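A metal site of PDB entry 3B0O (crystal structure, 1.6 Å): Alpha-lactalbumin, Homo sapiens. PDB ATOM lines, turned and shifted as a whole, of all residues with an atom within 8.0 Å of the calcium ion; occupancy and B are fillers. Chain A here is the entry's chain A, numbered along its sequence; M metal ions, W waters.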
ATOM      1  N   THR A  38     -24.048  19.158  25.186  1.00  0.00           N
ATOM      2  CA  THR A  38     -24.305  19.398  23.779  1.00  0.00           C
ATOM      3  C   THR A  38     -25.665  18.831  23.283  1.00  0.00           C
ATOM      4  O   THR A  38     -26.118  19.210  22.232  1.00  0.00           O
ATOM      5  CB  THR A  38     -23.226  18.861  22.865  1.00  0.00           C
ATOM      6  OG1 THR A  38     -23.253  17.424  22.865  1.00  0.00           O
ATOM      7  CG2 THR A  38     -21.844  19.372  23.241  1.00  0.00           C
ATOM      8  N   GLY A  51     -28.908  22.358  21.625  1.00  0.00           N
ATOM      9  CA  GLY A  51     -27.498  22.240  21.928  1.00  0.00           C
ATOM     10  C   GLY A  51     -26.934  23.383  22.753  1.00  0.00           C
ATOM     11  O   GLY A  51     -27.661  24.182  23.328  1.00  0.00           O
ATOM     12  N   LEU A  52     -25.617  23.420  22.846  1.00  0.00           N
ATOM     13  CA  LEU A  52     -24.958  24.401  23.705  1.00  0.00           C
ATOM     14  C   LEU A  52     -25.348  25.809  23.444  1.00  0.00           C
ATOM     15  O   LEU A  52     -25.530  26.621  24.397  1.00  0.00           O
ATOM     16  CB  LEU A  52     -23.461  24.291  23.591  1.00  0.00           C
ATOM     17  CG  LEU A  52     -22.668  23.890  24.771  1.00  0.00           C
ATOM     18  CD1 LEU A  52     -23.309  22.720  25.627  1.00  0.00           C
ATOM     19  CD2 LEU A  52     -21.212  23.657  24.224  1.00  0.00           C
ATOM     20  N   ILE A  75     -28.211  24.105   7.613  1.00  0.00           N
ATOM     21  CA  ILE A  75     -27.773  22.883   8.301  1.00  0.00           C
ATOM     22  C   ILE A  75     -28.956  22.235   9.012  1.00  0.00           C
ATOM     23  O   ILE A  75     -29.898  22.950   9.443  1.00  0.00           O
ATOM     24  CB  ILE A  75     -26.606  23.192   9.239  1.00  0.00           C
ATOM     25  CG1 ILE A  75     -25.862  21.969   9.645  1.00  0.00           C
ATOM     26  CG2 ILE A  75     -27.046  24.043  10.411  1.00  0.00           C
ATOM     27  CD1 ILE A  75     -24.589  22.276  10.449  1.00  0.00           C
ATOM     28  N   SER A  76     -28.927  20.893   9.103  1.00  0.00           N
ATOM     29  CA  SER A  76     -29.899  20.212   9.951  1.00  0.00           C
ATOM     30  C   SER A  76     -29.726  20.538  11.391  1.00  0.00           C
ATOM     31  O   SER A  76     -28.567  20.493  11.891  1.00  0.00           O
ATOM     32  CB  SER A  76     -29.826  18.693   9.775  1.00  0.00           C
ATOM     33  OG  SER A  76     -30.720  18.038  10.665  1.00  0.00           O
ATOM     34  N   CYS A  77     -30.806  20.800  12.164  1.00  0.00           N
ATOM     35  CA  CYS A  77     -30.689  21.114  13.576  1.00  0.00           C
ATOM     36  C   CYS A  77     -30.033  19.902  14.338  1.00  0.00           C
ATOM     37  O   CYS A  77     -29.546  20.123  15.420  1.00  0.00           O
ATOM     38  CB  CYS A  77     -32.053  21.382  14.207  1.00  0.00           C
ATOM     39  SG  CYS A  77     -32.956  22.758  13.472  1.00  0.00           S
ATOM     40  N   ASP A  78     -30.073  18.673  13.789  1.00  0.00           N
ATOM     41  CA  ASP A  78     -29.536  17.516  14.480  1.00  0.00           C
ATOM     42  C   ASP A  78     -28.031  17.727  14.731  1.00  0.00           C
ATOM     43  O   ASP A  78     -27.496  17.235  15.747  1.00  0.00           O
ATOM     44  CB  ASP A  78     -29.795  16.200  13.718  1.00  0.00           C
ATOM     45  CG  ASP A  78     -28.756  15.880  12.659  1.00  0.00           C
ATOM     46  OD1 ASP A  78     -28.990  16.192  11.517  1.00  0.00           O
ATOM     47  OD2 ASP A  78     -27.669  15.349  12.981  1.00  0.00           O
ATOM     48  N   LYS A  79     -27.426  18.524  13.799  1.00  0.00           N
ATOM     49  CA  LYS A  79     -25.977  18.714  13.981  1.00  0.00           C
ATOM     50  C   LYS A  79     -25.681  19.448  15.289  1.00  0.00           C
ATOM     51  O   LYS A  79     -24.534  19.322  15.843  1.00  0.00           O
ATOM     52  CB  LYS A  79     -25.434  19.500  12.841  1.00  0.00           C
ATOM     53  CG  LYS A  79     -25.155  18.581  11.610  1.00  0.00           C
ATOM     54  CD  LYS A  79     -23.952  17.633  11.847  1.00  0.00           C
ATOM     55  CE  LYS A  79     -22.639  18.366  11.799  1.00  0.00           C
ATOM     56  NZ  LYS A  79     -21.532  17.547  12.373  1.00  0.00           N
ATOM     57  N   PHE A  80     -26.642  20.174  15.833  1.00  0.00           N
ATOM     58  CA  PHE A  80     -26.443  20.902  17.086  1.00  0.00           C
ATOM     59  C   PHE A  80     -26.644  20.058  18.366  1.00  0.00           C
ATOM     60  O   PHE A  80     -26.503  20.570  19.464  1.00  0.00           O
ATOM     61  CB  PHE A  80     -27.283  22.128  17.149  1.00  0.00           C
ATOM     62  CG  PHE A  80     -27.157  23.048  15.953  1.00  0.00           C
ATOM     63  CD1 PHE A  80     -25.955  23.279  15.365  1.00  0.00           C
ATOM     64  CD2 PHE A  80     -28.246  23.741  15.463  1.00  0.00           C
ATOM     65  CE1 PHE A  80     -25.805  24.130  14.263  1.00  0.00           C
ATOM     66  CE2 PHE A  80     -28.090  24.677  14.412  1.00  0.00           C
ATOM     67  CZ  PHE A  80     -26.827  24.825  13.842  1.00  0.00           C
ATOM     68  N   LEU A  81     -26.822  18.781  18.177  1.00  0.00           N
ATOM     69  CA  LEU A  81     -26.948  17.806  19.265  1.00  0.00           C
ATOM     70  C   LEU A  81     -25.836  16.780  19.303  1.00  0.00           C
ATOM     71  O   LEU A  81     -25.827  15.890  20.164  1.00  0.00           O
ATOM     72  CB  LEU A  81     -28.311  17.099  19.212  1.00  0.00           C
ATOM     73  CG  LEU A  81     -29.499  17.965  19.342  1.00  0.00           C
ATOM     74  CD1 LEU A  81     -30.797  17.082  19.322  1.00  0.00           C
ATOM     75  CD2 LEU A  81     -29.497  18.865  20.630  1.00  0.00           C
ATOM     76  N   ASP A  82     -24.873  16.872  18.380  1.00  0.00           N
ATOM     77  CA  ASP A  82     -23.750  15.928  18.364  1.00  0.00           C
ATOM     78  C   ASP A  82     -22.627  16.374  19.342  1.00  0.00           C
ATOM     79  O   ASP A  82     -22.776  17.439  20.028  1.00  0.00           O
ATOM     80  CB  ASP A  82     -23.332  15.614  16.952  1.00  0.00           C
ATOM     81  CG  ASP A  82     -22.632  16.717  16.188  1.00  0.00           C
ATOM     82  OD1 ASP A  82     -22.214  17.724  16.806  1.00  0.00           O
ATOM     83  OD2 ASP A  82     -22.624  16.635  14.907  1.00  0.00           O
ATOM     84  N   ASP A  83     -21.491  15.689  19.357  1.00  0.00           N
ATOM     85  CA  ASP A  83     -20.406  16.008  20.241  1.00  0.00           C
ATOM     86  C   ASP A  83     -19.391  17.041  19.709  1.00  0.00           C
ATOM     87  O   ASP A  83     -18.444  17.299  20.396  1.00  0.00           O
ATOM     88  CB  ASP A  83     -19.640  14.724  20.639  1.00  0.00           C
ATOM     89  CG  ASP A  83     -18.872  14.082  19.477  1.00  0.00           C
ATOM     90  OD1 ASP A  83     -18.873  14.551  18.284  1.00  0.00           O
ATOM     91  OD2 ASP A  83     -18.259  12.959  19.735  1.00  0.00           O
ATOM     92  N   ASP A  84     -19.678  17.660  18.578  1.00  0.00           N
ATOM     93  CA  ASP A  84     -18.711  18.531  17.820  1.00  0.00           C
ATOM     94  C   ASP A  84     -19.385  19.880  17.833  1.00  0.00           C
ATOM     95  O   ASP A  84     -20.337  20.125  17.062  1.00  0.00           O
ATOM     96  CB  ASP A  84     -18.488  17.969  16.470  1.00  0.00           C
ATOM     97  CG  ASP A  84     -17.558  18.858  15.628  1.00  0.00           C
ATOM     98  OD1 ASP A  84     -16.995  19.778  16.300  1.00  0.00           O
ATOM     99  OD2 ASP A  84     -17.457  18.683  14.419  1.00  0.00           O
ATOM    100  N   ILE A  85     -18.874  20.790  18.657  1.00  0.00           N
ATOM    101  CA  ILE A  85     -19.489  22.115  18.710  1.00  0.00           C
ATOM    102  C   ILE A  85     -18.980  23.051  17.568  1.00  0.00           C
ATOM    103  O   ILE A  85     -19.409  24.206  17.537  1.00  0.00           O
ATOM    104  CB  ILE A  85     -19.442  22.763  20.105  1.00  0.00           C
ATOM    105  CG1 ILE A  85     -18.075  23.152  20.502  1.00  0.00           C
ATOM    106  CG2 ILE A  85     -20.098  21.836  21.075  1.00  0.00           C
ATOM    107  CD1 ILE A  85     -18.015  23.951  21.832  1.00  0.00           C
ATOM    108  N   THR A  86     -18.167  22.537  16.632  1.00  0.00           N
ATOM    109  CA  THR A  86     -17.699  23.355  15.485  1.00  0.00           C
ATOM    110  C   THR A  86     -18.785  23.959  14.621  1.00  0.00           C
ATOM    111  O   THR A  86     -18.798  25.164  14.368  1.00  0.00           O
ATOM    112  CB  THR A  86     -16.756  22.516  14.655  1.00  0.00           C
ATOM    113  OG1 THR A  86     -15.624  22.187  15.478  1.00  0.00           O
ATOM    114  CG2 THR A  86     -16.316  23.240  13.452  1.00  0.00           C
ATOM    115  N   ASP A  87     -19.729  23.135  14.229  1.00  0.00           N
ATOM    116  CA  ASP A  87     -20.873  23.628  13.417  1.00  0.00           C
ATOM    117  C   ASP A  87     -21.761  24.571  14.235  1.00  0.00           C
ATOM    118  O   ASP A  87     -22.319  25.540  13.682  1.00  0.00           O
ATOM    119  CB  ASP A  87     -21.658  22.426  12.865  1.00  0.00           C
ATOM    120  CG  ASP A  87     -22.118  21.543  13.995  1.00  0.00           C
ATOM    121  OD1 ASP A  87     -23.330  21.603  14.412  1.00  0.00           O
ATOM    122  OD2 ASP A  87     -21.343  20.785  14.486  1.00  0.00           O
ATOM    123  N   ASP A  88     -21.911  24.342  15.547  1.00  0.00           N
ATOM    124  CA  ASP A  88     -22.688  25.156  16.426  1.00  0.00           C
ATOM    125  C   ASP A  88     -22.057  26.550  16.491  1.00  0.00           C
ATOM    126  O   ASP A  88     -22.755  27.573  16.434  1.00  0.00           O
ATOM    127  CB  ASP A  88     -22.815  24.526  17.837  1.00  0.00           C
ATOM    128  CG  ASP A  88     -23.238  23.124  17.857  1.00  0.00           C
ATOM    129  OD1 ASP A  88     -22.639  22.252  17.261  1.00  0.00           O
ATOM    130  OD2 ASP A  88     -24.182  22.878  18.655  1.00  0.00           O
ATOM    131  N   ILE A  89     -20.722  26.601  16.671  1.00  0.00           N
ATOM    132  CA  ILE A  89     -20.014  27.868  16.639  1.00  0.00           C
ATOM    133  C   ILE A  89     -20.199  28.609  15.316  1.00  0.00           C
ATOM    134  O   ILE A  89     -20.412  29.805  15.314  1.00  0.00           O
ATOM    135  CB  ILE A  89     -18.500  27.668  16.971  1.00  0.00           C
ATOM    136  CG1 ILE A  89     -18.330  27.158  18.392  1.00  0.00           C
ATOM    137  CG2 ILE A  89     -17.794  29.050  16.814  1.00  0.00           C
ATOM    138  CD1 ILE A  89     -16.980  26.450  18.622  1.00  0.00           C
HETATM  139 CA    CA M   1     -22.487  20.081  16.413  1.00  0.00          CA
HETATM  140  O   HOH W   1     -23.088  19.818  18.791  1.00  0.00           O
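The side-chain carboxylate (OD1) of Asp 84 is in hydrogen-bond range of the side-chain hydroxyl (OG1) of Thr 86 (2.9 Å).
The side-chain hydroxyl (OG1) of Thr 38 lies within hydrogen-bond range of the backbone carbonyl oxygen (O) of Asp 82 (2.9 Å).
Of the 18 residues printed, 5 come within 4 Å of the calcium ion.
The nearest printed residue that does not touch the calcium ion is Phe 80 (4.1 Å).
The calcium ion is bound by the backbone carbonyl oxygen (O) of Asp 84 (2.2 Å), the backbone carbonyl oxygen (O) of Lys 79 (2.3 Å), the side-chain carboxylate (OD1) of Asp 88 (2.3 Å), the side-chain carboxylate (OD2) of Asp 87 (2.3 Å), the side-chain carboxylate (OD1) of Asp 82 (2.4 Å), water W1 (2.5 Å) and the side-chain carboxylate (OD1) of Asp 87 (2.7 Å).
Water W1 lies within hydrogen-bond range of the backbone carbonyl oxygen (O) of Asp 82 (2.7 Å) and the side-chain carboxylate (OD2) of Asp 88 (3.3 Å).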
